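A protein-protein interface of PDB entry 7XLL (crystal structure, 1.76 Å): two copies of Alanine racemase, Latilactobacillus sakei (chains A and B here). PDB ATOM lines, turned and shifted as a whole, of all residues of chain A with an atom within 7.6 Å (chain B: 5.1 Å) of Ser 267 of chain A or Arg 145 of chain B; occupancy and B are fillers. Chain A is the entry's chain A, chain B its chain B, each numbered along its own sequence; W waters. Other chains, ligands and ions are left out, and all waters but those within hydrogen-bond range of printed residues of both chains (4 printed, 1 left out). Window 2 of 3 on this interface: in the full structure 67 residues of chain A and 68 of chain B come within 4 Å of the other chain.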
ATOM      1  N   PHE A 259      19.680  14.149 -12.607  1.00  0.00           N
ATOM      2  CA  PHE A 259      20.161  13.179 -11.638  1.00  0.00           C
ATOM      3  C   PHE A 259      20.741  12.007 -12.414  1.00  0.00           C
ATOM      4  O   PHE A 259      20.144  11.561 -13.394  1.00  0.00           O
ATOM      5  CB  PHE A 259      19.031  12.711 -10.706  1.00  0.00           C
ATOM      6  CG  PHE A 259      19.517  12.236  -9.357  1.00  0.00           C
ATOM      7  CD1 PHE A 259      19.669  13.132  -8.312  1.00  0.00           C
ATOM      8  CD2 PHE A 259      19.834  10.900  -9.142  1.00  0.00           C
ATOM      9  CE1 PHE A 259      20.126  12.703  -7.065  1.00  0.00           C
ATOM     10  CE2 PHE A 259      20.282  10.459  -7.897  1.00  0.00           C
ATOM     11  CZ  PHE A 259      20.428  11.372  -6.855  1.00  0.00           C
ATOM     12  N   LYS A 261      22.828   8.189 -11.680  1.00  0.00           N
ATOM     13  CA  LYS A 261      23.271   7.224 -10.684  1.00  0.00           C
ATOM     14  C   LYS A 261      23.515   5.880 -11.349  1.00  0.00           C
ATOM     15  O   LYS A 261      22.947   5.568 -12.400  1.00  0.00           O
ATOM     16  CB  LYS A 261      22.238   7.065  -9.563  1.00  0.00           C
ATOM     17  CG  LYS A 261      20.867   6.629 -10.079  1.00  0.00           C
ATOM     18  CD  LYS A 261      19.975   6.160  -8.959  1.00  0.00           C
ATOM     19  CE  LYS A 261      18.536   5.998  -9.432  1.00  0.00           C
ATOM     20  NZ  LYS A 261      17.871   7.316  -9.689  1.00  0.00           N
ATOM     21  N   GLN A 262      24.369   5.083 -10.716  1.00  0.00           N
ATOM     22  CA  GLN A 262      24.618   3.708 -11.125  1.00  0.00           C
ATOM     23  C   GLN A 262      24.023   2.774 -10.083  1.00  0.00           C
ATOM     24  O   GLN A 262      24.169   3.009  -8.877  1.00  0.00           O
ATOM     25  CB  GLN A 262      26.118   3.437 -11.275  1.00  0.00           C
ATOM     26  CG  GLN A 262      26.444   2.052 -11.846  1.00  0.00           C
ATOM     27  CD  GLN A 262      27.932   1.853 -12.021  1.00  0.00           C
ATOM     28  OE1 GLN A 262      28.726   2.193 -11.134  1.00  0.00           O
ATOM     29  NE2 GLN A 262      28.327   1.322 -13.174  1.00  0.00           N
ATOM     30  N   VAL A 263      23.349   1.714 -10.538  1.00  0.00           N
ATOM     31  CA  VAL A 263      22.581   0.873  -9.628  1.00  0.00           C
ATOM     32  C   VAL A 263      22.977  -0.593  -9.770  1.00  0.00           C
ATOM     33  O   VAL A 263      23.553  -1.018 -10.775  1.00  0.00           O
ATOM     34  CB  VAL A 263      21.063   1.041  -9.835  1.00  0.00           C
ATOM     35  CG1 VAL A 263      20.690   2.516  -9.679  1.00  0.00           C
ATOM     36  CG2 VAL A 263      20.642   0.523 -11.194  1.00  0.00           C
ATOM     37  N   ALA A 264      22.667  -1.360  -8.728  1.00  0.00           N
ATOM     38  CA  ALA A 264      22.949  -2.789  -8.667  1.00  0.00           C
ATOM     39  C   ALA A 264      21.853  -3.591  -9.373  1.00  0.00           C
ATOM     40  O   ALA A 264      20.730  -3.118  -9.553  1.00  0.00           O
ATOM     41  CB  ALA A 264      23.071  -3.232  -7.209  1.00  0.00           C
ATOM     42  N   ALA A 265      22.186  -4.827  -9.759  1.00  0.00           N
ATOM     43  CA  ALA A 265      21.204  -5.686 -10.413  1.00  0.00           C
ATOM     44  C   ALA A 265      19.976  -5.879  -9.527  1.00  0.00           C
ATOM     45  O   ALA A 265      20.080  -6.041  -8.307  1.00  0.00           O
ATOM     46  CB  ALA A 265      21.829  -7.041 -10.759  1.00  0.00           C
ATOM     47  N   GLY A 266      18.801  -5.848 -10.150  1.00  0.00           N
ATOM     48  CA  GLY A 266      17.547  -6.000  -9.445  1.00  0.00           C
ATOM     49  C   GLY A 266      16.948  -4.723  -8.895  1.00  0.00           C
ATOM     50  O   GLY A 266      15.825  -4.767  -8.362  1.00  0.00           O
ATOM     51  N   SER A 267      17.654  -3.594  -8.988  1.00  0.00           N
ATOM     52  CA  SER A 267      17.107  -2.336  -8.493  1.00  0.00           C
ATOM     53  C   SER A 267      15.839  -1.976  -9.257  1.00  0.00           C
ATOM     54  O   SER A 267      15.840  -1.919 -10.487  1.00  0.00           O
ATOM     55  CB  SER A 267      18.141  -1.208  -8.620  1.00  0.00           C
ATOM     56  OG  SER A 267      19.326  -1.501  -7.899  1.00  0.00           O
ATOM     57  N   LYS A 268      14.759  -1.739  -8.519  1.00  0.00           N
ATOM     58  CA  LYS A 268      13.461  -1.435  -9.107  1.00  0.00           C
ATOM     59  C   LYS A 268      13.365   0.061  -9.378  1.00  0.00           C
ATOM     60  O   LYS A 268      13.774   0.877  -8.544  1.00  0.00           O
ATOM     61  CB  LYS A 268      12.338  -1.902  -8.172  1.00  0.00           C
ATOM     62  CG  LYS A 268      12.395  -3.427  -7.941  1.00  0.00           C
ATOM     63  CD  LYS A 268      11.468  -3.929  -6.836  1.00  0.00           C
ATOM     64  CE  LYS A 268      11.526  -5.463  -6.755  1.00  0.00           C
ATOM     65  NZ  LYS A 268      10.735  -6.055  -5.626  1.00  0.00           N
ATOM     66  N   ILE A 269      12.834   0.418 -10.549  1.00  0.00           N
ATOM     67  CA  ILE A 269      12.790   1.814 -11.002  1.00  0.00           C
ATOM     68  C   ILE A 269      11.342   2.213 -11.267  1.00  0.00           C
ATOM     69  O   ILE A 269      10.659   1.586 -12.085  1.00  0.00           O
ATOM     70  CB  ILE A 269      13.636   2.040 -12.266  1.00  0.00           C
ATOM     71  CG1 ILE A 269      15.083   1.572 -12.074  1.00  0.00           C
ATOM     72  CG2 ILE A 269      13.561   3.520 -12.701  1.00  0.00           C
ATOM     73  CD1 ILE A 269      15.830   2.270 -10.943  1.00  0.00           C
ATOM     74  N   GLY A 270      10.888   3.280 -10.598  1.00  0.00           N
ATOM     75  CA  GLY A 270       9.629   3.924 -10.913  1.00  0.00           C
ATOM     76  C   GLY A 270       8.420   3.339 -10.213  1.00  0.00           C
ATOM     77  O   GLY A 270       8.477   2.330  -9.501  1.00  0.00           O
ATOM     78  N   ALA A 273       7.244  -0.420  -9.532  1.00  0.00           N
ATOM     79  CA  ALA A 273       8.467  -1.221  -9.639  1.00  0.00           C
ATOM     80  C   ALA A 273       8.474  -2.079 -10.905  1.00  0.00           C
ATOM     81  O   ALA A 273       8.919  -3.234 -10.898  1.00  0.00           O
ATOM     82  CB  ALA A 273       8.665  -2.083  -8.389  1.00  0.00           C
ATOM     83  N   TYR A 275      10.177  -1.966 -13.638  1.00  0.00           N
ATOM     84  CA  TYR A 275      11.429  -2.188 -14.345  1.00  0.00           C
ATOM     85  C   TYR A 275      12.507  -2.541 -13.333  1.00  0.00           C
ATOM     86  O   TYR A 275      12.598  -1.916 -12.273  1.00  0.00           O
ATOM     87  CB  TYR A 275      11.843  -0.952 -15.158  1.00  0.00           C
ATOM     88  CG  TYR A 275      13.196  -1.078 -15.825  1.00  0.00           C
ATOM     89  CD1 TYR A 275      13.322  -1.686 -17.074  1.00  0.00           C
ATOM     90  CD2 TYR A 275      14.347  -0.582 -15.216  1.00  0.00           C
ATOM     91  CE1 TYR A 275      14.559  -1.804 -17.689  1.00  0.00           C
ATOM     92  CE2 TYR A 275      15.586  -0.699 -15.820  1.00  0.00           C
ATOM     93  CZ  TYR A 275      15.689  -1.308 -17.053  1.00  0.00           C
ATOM     94  OH  TYR A 275      16.918  -1.433 -17.660  1.00  0.00           O
ATOM     95  N   GLU A 276      13.320  -3.548 -13.653  1.00  0.00           N
ATOM     96  CA  GLU A 276      14.431  -3.948 -12.790  1.00  0.00           C
ATOM     97  C   GLU A 276      15.736  -3.804 -13.556  1.00  0.00           C
ATOM     98  O   GLU A 276      15.892  -4.381 -14.637  1.00  0.00           O
ATOM     99  CB  GLU A 276      14.256  -5.386 -12.285  1.00  0.00           C
ATOM    100  CG  GLU A 276      13.179  -5.485 -11.226  1.00  0.00           C
ATOM    101  CD  GLU A 276      13.066  -6.852 -10.598  1.00  0.00           C
ATOM    102  OE1 GLU A 276      11.996  -7.123 -10.014  1.00  0.00           O
ATOM    103  OE2 GLU A 276      14.035  -7.644 -10.671  1.00  0.00           O
ATOM    104  N   ALA A 277      16.675  -3.049 -12.993  1.00  0.00           N
ATOM    105  CA  ALA A 277      17.926  -2.790 -13.688  1.00  0.00           C
ATOM    106  C   ALA A 277      18.851  -4.007 -13.670  1.00  0.00           C
ATOM    107  O   ALA A 277      18.758  -4.892 -12.812  1.00  0.00           O
ATOM    108  CB  ALA A 277      18.649  -1.599 -13.060  1.00  0.00           C
ATOM    109  N   SER A 278      19.760  -4.033 -14.645  1.00  0.00           N
ATOM    110  CA  SER A 278      20.891  -4.947 -14.653  1.00  0.00           C
ATOM    111  C   SER A 278      22.040  -4.389 -13.818  1.00  0.00           C
ATOM    112  O   SER A 278      22.021  -3.241 -13.359  1.00  0.00           O
ATOM    113  CB  SER A 278      21.368  -5.221 -16.082  1.00  0.00           C
ATOM    114  OG  SER A 278      20.277  -5.360 -16.976  1.00  0.00           O
ATOM    115  N   GLU A 279      23.068  -5.213 -13.637  1.00  0.00           N
ATOM    116  CA  GLU A 279      24.181  -4.816 -12.784  1.00  0.00           C
ATOM    117  C   GLU A 279      24.934  -3.638 -13.392  1.00  0.00           C
ATOM    118  O   GLU A 279      25.314  -3.666 -14.567  1.00  0.00           O
ATOM    119  CB  GLU A 279      25.132  -5.995 -12.564  1.00  0.00           C
ATOM    120  CG  GLU A 279      26.291  -5.680 -11.622  1.00  0.00           C
ATOM    121  CD  GLU A 279      25.819  -5.223 -10.256  1.00  0.00           C
ATOM    122  OE1 GLU A 279      24.848  -5.804  -9.737  1.00  0.00           O
ATOM    123  OE2 GLU A 279      26.413  -4.273  -9.706  1.00  0.00           O
ATOM    124  N   GLY A 280      25.143  -2.593 -12.592  1.00  0.00           N
ATOM    125  CA  GLY A 280      25.955  -1.471 -13.037  1.00  0.00           C
ATOM    126  C   GLY A 280      25.266  -0.549 -14.011  1.00  0.00           C
ATOM    127  O   GLY A 280      25.927   0.251 -14.681  1.00  0.00           O
ATOM    128  N   GLU A 281      23.950  -0.660 -14.124  1.00  0.00           N
ATOM    129  CA  GLU A 281      23.204   0.153 -15.063  1.00  0.00           C
ATOM    130  C   GLU A 281      23.231   1.613 -14.631  1.00  0.00           C
ATOM    131  O   GLU A 281      23.136   1.925 -13.442  1.00  0.00           O
ATOM    132  CB  GLU A 281      21.769  -0.349 -15.140  1.00  0.00           C
ATOM    133  CG  GLU A 281      21.024   0.087 -16.349  1.00  0.00           C
ATOM    134  CD  GLU A 281      19.746  -0.699 -16.501  1.00  0.00           C
ATOM    135  OE1 GLU A 281      18.663  -0.112 -16.344  1.00  0.00           O
ATOM    136  OE2 GLU A 281      19.830  -1.912 -16.749  1.00  0.00           O
ATOM    137  N   ILE A 283      21.304   5.126 -14.643  1.00  0.00           N
ATOM    138  CA  ILE A 283      19.935   5.629 -14.742  1.00  0.00           C
ATOM    139  C   ILE A 283      19.985   7.147 -14.678  1.00  0.00           C
ATOM    140  O   ILE A 283      20.554   7.706 -13.733  1.00  0.00           O
ATOM    141  CB  ILE A 283      19.034   5.069 -13.624  1.00  0.00           C
ATOM    142  CG1 ILE A 283      19.022   3.536 -13.655  1.00  0.00           C
ATOM    143  CG2 ILE A 283      17.610   5.648 -13.740  1.00  0.00           C
ATOM    144  CD1 ILE A 283      18.371   2.977 -14.873  1.00  0.00           C
ATOM    145  N   ASP B 136      16.385   8.049  -1.666  1.00  0.00           N
ATOM    146  CA  ASP B 136      15.848   7.058  -2.599  1.00  0.00           C
ATOM    147  C   ASP B 136      15.836   5.732  -1.851  1.00  0.00           C
ATOM    148  O   ASP B 136      16.864   5.067  -1.727  1.00  0.00           O
ATOM    149  CB  ASP B 136      16.693   6.995  -3.867  1.00  0.00           C
ATOM    150  CG  ASP B 136      16.220   5.919  -4.854  1.00  0.00           C
ATOM    151  OD1 ASP B 136      15.239   5.202  -4.562  1.00  0.00           O
ATOM    152  OD2 ASP B 136      16.832   5.808  -5.943  1.00  0.00           O
ATOM    153  N   GLY B 138      14.051   3.179  -2.843  1.00  0.00           N
ATOM    154  CA  GLY B 138      13.647   2.105  -3.735  1.00  0.00           C
ATOM    155  C   GLY B 138      12.727   2.534  -4.856  1.00  0.00           C
ATOM    156  O   GLY B 138      12.284   1.698  -5.649  1.00  0.00           O
ATOM    157  N   GLY B 140      13.876   4.661  -7.065  1.00  0.00           N
ATOM    158  CA  GLY B 140      14.834   4.767  -8.148  1.00  0.00           C
ATOM    159  C   GLY B 140      14.777   6.052  -8.942  1.00  0.00           C
ATOM    160  O   GLY B 140      15.358   6.114 -10.029  1.00  0.00           O
ATOM    161  N   GLY B 143      17.537  10.935  -5.318  1.00  0.00           N
ATOM    162  CA  GLY B 143      17.831  10.837  -3.900  1.00  0.00           C
ATOM    163  C   GLY B 143      19.010   9.977  -3.489  1.00  0.00           C
ATOM    164  O   GLY B 143      19.475   9.129  -4.256  1.00  0.00           O
ATOM    165  N   PHE B 144      19.492  10.190  -2.264  1.00  0.00           N
ATOM    166  CA  PHE B 144      20.615   9.420  -1.738  1.00  0.00           C
ATOM    167  C   PHE B 144      20.256   7.947  -1.655  1.00  0.00           C
ATOM    168  O   PHE B 144      19.137   7.599  -1.271  1.00  0.00           O
ATOM    169  CB  PHE B 144      20.997   9.925  -0.344  1.00  0.00           C
ATOM    170  CG  PHE B 144      21.442  11.365  -0.331  1.00  0.00           C
ATOM    171  CD1 PHE B 144      22.785  11.685  -0.476  1.00  0.00           C
ATOM    172  CD2 PHE B 144      20.520  12.389  -0.205  1.00  0.00           C
ATOM    173  CE1 PHE B 144      23.205  13.005  -0.480  1.00  0.00           C
ATOM    174  CE2 PHE B 144      20.936  13.709  -0.221  1.00  0.00           C
ATOM    175  CZ  PHE B 144      22.286  14.010  -0.349  1.00  0.00           C
ATOM    176  N   ARG B 145      21.221   7.084  -1.999  1.00  0.00           N
ATOM    177  CA  ARG B 145      21.034   5.635  -1.940  1.00  0.00           C
ATOM    178  C   ARG B 145      22.014   4.939  -1.000  1.00  0.00           C
ATOM    179  O   ARG B 145      22.014   3.704  -0.931  1.00  0.00           O
ATOM    180  CB  ARG B 145      21.132   5.024  -3.348  1.00  0.00           C
ATOM    181  CG  ARG B 145      19.925   5.362  -4.225  1.00  0.00           C
ATOM    182  CD  ARG B 145      20.085   4.906  -5.685  1.00  0.00           C
ATOM    183  NE  ARG B 145      20.115   3.453  -5.860  1.00  0.00           N
ATOM    184  CZ  ARG B 145      19.040   2.681  -6.053  1.00  0.00           C
ATOM    185  NH1 ARG B 145      17.817   3.201  -6.073  1.00  0.00           N
ATOM    186  NH2 ARG B 145      19.188   1.371  -6.215  1.00  0.00           N
ATOM    187  N   ASP B 146      22.839   5.676  -0.256  1.00  0.00           N
ATOM    188  CA  ASP B 146      23.767   5.002   0.644  1.00  0.00           C
ATOM    189  C   ASP B 146      24.096   5.884   1.842  1.00  0.00           C
ATOM    190  O   ASP B 146      24.002   7.114   1.793  1.00  0.00           O
ATOM    191  CB  ASP B 146      25.055   4.572  -0.073  1.00  0.00           C
ATOM    192  CG  ASP B 146      25.890   5.744  -0.524  1.00  0.00           C
ATOM    193  OD1 ASP B 146      25.486   6.406  -1.502  1.00  0.00           O
ATOM    194  OD2 ASP B 146      26.949   6.006   0.095  1.00  0.00           O
ATOM    195  N   GLU B 147      24.516   5.206   2.911  1.00  0.00           N
ATOM    196  CA  GLU B 147      24.738   5.861   4.197  1.00  0.00           C
ATOM    197  C   GLU B 147      25.834   6.917   4.110  1.00  0.00           C
ATOM    198  O   GLU B 147      25.689   8.020   4.654  1.00  0.00           O
ATOM    199  CB  GLU B 147      25.099   4.811   5.252  1.00  0.00           C
ATOM    200  CG  GLU B 147      23.999   3.787   5.561  1.00  0.00           C
ATOM    201  CD  GLU B 147      23.881   2.657   4.530  1.00  0.00           C
ATOM    202  OE1 GLU B 147      24.457   2.762   3.420  1.00  0.00           O
ATOM    203  OE2 GLU B 147      23.200   1.652   4.835  1.00  0.00           O
ATOM    204  N   ARG B 190      14.203   0.549   4.742  1.00  0.00           N
ATOM    205  CA  ARG B 190      15.426   1.138   4.204  1.00  0.00           C
ATOM    206  C   ARG B 190      15.533   2.622   4.545  1.00  0.00           C
ATOM    207  O   ARG B 190      16.614   3.104   4.903  1.00  0.00           O
ATOM    208  CB  ARG B 190      15.483   0.926   2.692  1.00  0.00           C
ATOM    209  CG  ARG B 190      16.658   1.597   2.006  1.00  0.00           C
ATOM    210  CD  ARG B 190      17.988   1.167   2.607  1.00  0.00           C
ATOM    211  NE  ARG B 190      19.114   1.627   1.800  1.00  0.00           N
ATOM    212  CZ  ARG B 190      20.367   1.695   2.236  1.00  0.00           C
ATOM    213  NH1 ARG B 190      20.662   1.330   3.477  1.00  0.00           N
ATOM    214  NH2 ARG B 190      21.328   2.131   1.431  1.00  0.00           N
ATOM    215  N   LEU B 194      18.356   4.543   6.981  1.00  0.00           N
ATOM    216  CA  LEU B 194      19.211   5.661   6.587  1.00  0.00           C
ATOM    217  C   LEU B 194      18.995   6.873   7.485  1.00  0.00           C
ATOM    218  O   LEU B 194      19.959   7.558   7.845  1.00  0.00           O
ATOM    219  CB  LEU B 194      18.982   6.009   5.114  1.00  0.00           C
ATOM    220  CG  LEU B 194      19.550   4.990   4.114  1.00  0.00           C
ATOM    221  CD1 LEU B 194      18.975   5.183   2.733  1.00  0.00           C
ATOM    222  CD2 LEU B 194      21.056   5.073   4.044  1.00  0.00           C
HETATM  223  O   HOH W   1      21.998   0.089  -6.169  1.00  0.00           O
HETATM  224  O   HOH W   2      22.997   3.416  -6.487  1.00  0.00           O
HETATM  225  O   HOH W   3      15.747   1.237  -6.662  1.00  0.00           O
HETATM  226  O   HOH W   4      17.929   8.055  -6.923  1.00  0.00           O
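The side-chain amino group of Lys 261 of chain A lies within hydrogen-bond range of the backbone carbonyl oxygen of Gly 140 of chain B, 2.8 Å away. OG of Ser 267 of chain A sits at hydrogen-bond distance from NH2 of Arg 145 of chain B, 3.3 Å away. The backbone carbonyl oxygen (O) of Lys 268 of chain A sits close to the backbone carbonyl oxygen (O) of Gly 138 of chain B.
The backbone carbonyl oxygen (O) of Val 263 of chain A lies within hydrogen-bond range of the backbone NH (N) of Gly 280 of chain A, at 2.9 Å. N of Ala 277 of chain A sits at hydrogen-bond distance from O of Ser 267 of chain A (2.9 Å). The backbone carbonyl oxygen of Tyr 275 of chain A sits at hydrogen-bond distance from the backbone NH of Ile 269 of chain A, at 2.9 Å. The side-chain carboxylate (OD1) of Asp 136 of chain B sits at hydrogen-bond distance from the backbone NH (N) of Gly 140 of chain B (2.9 Å). The side-chain carboxylate of Asp 136 of chain B lies within salt-bridge range of the guanidinium group of Arg 145 of chain B (2.8 Å). The backbone carbonyl oxygen of Arg 145 of chain B sits at hydrogen-bond distance from the guanidinium group of Arg 190 of chain B (2.9 Å).
CZ of Phe 259 of chain A touches N of Gly 143 of chain B, 3.3 Å away. Lys 261 of chain A touches Asp 136 of chain B. Lys 261 of chain A touches Arg 145 of chain B. Val 263 of chain A touches Arg 145 of chain B (CG1 to NH2, 3.9 Å). Gly 140 of chain B touches Ile 269 of chain A.
Of chain B, only Arg 145 comes within 4 Å of Ser 267 of chain A. Of the printed residues of chain A, Gly 138 of chain B touches Lys 268 (3.4 Å). Of the printed residues of chain A, Gly 140 of chain B touches Lys 261 and Ile 269. Arg 145 of chain B touches three residues of chain A. The nearest printed residue of chain A that does not touch Arg 145 of chain B is Gln 262 of chain A (5.1 Å). The nearest printed residue of chain A that does not touch Gly 143 of chain B is Lys 261 of chain A (5.6 Å).
Of the 10 printed residues of chain B, 5 touch a printed residue of chain A. Printed residues of chain B that touch a printed residue of chain A: Asp 136, Gly 138, Gly 140, Gly 143 and Arg 145. Along chain B the printed residues that touch a printed residue of chain A span positions 136 to 145. Of the 20 printed residues of chain A, 6 touch a printed residue of chain B. Among the printed residues, no Asp or Glu carboxylate lies within 4 Å of a Lys or Arg side-chain nitrogen of the other chain.
No position is printed for both chains.
Water W4 lies within hydrogen-bond range of OD2 of Asp 136 of chain B (2.7 Å), NZ of Lys 261 of chain A (2.9 Å) and O of Gly 143 of chain B (3.3 Å). Water W2 bridges O of Gln 262 of chain A (2.7 Å) and NE of Arg 145 of chain B (2.9 Å). Water W3 lies within hydrogen-bond range of O of Lys 268 of chain A (2.8 Å) and NH1 of Arg 145 of chain B (2.9 Å). Water W1 lies within hydrogen-bond range of N of Ala 264 of chain A (3.0 Å) and NH2 of Arg 145 of chain B (3.1 Å).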
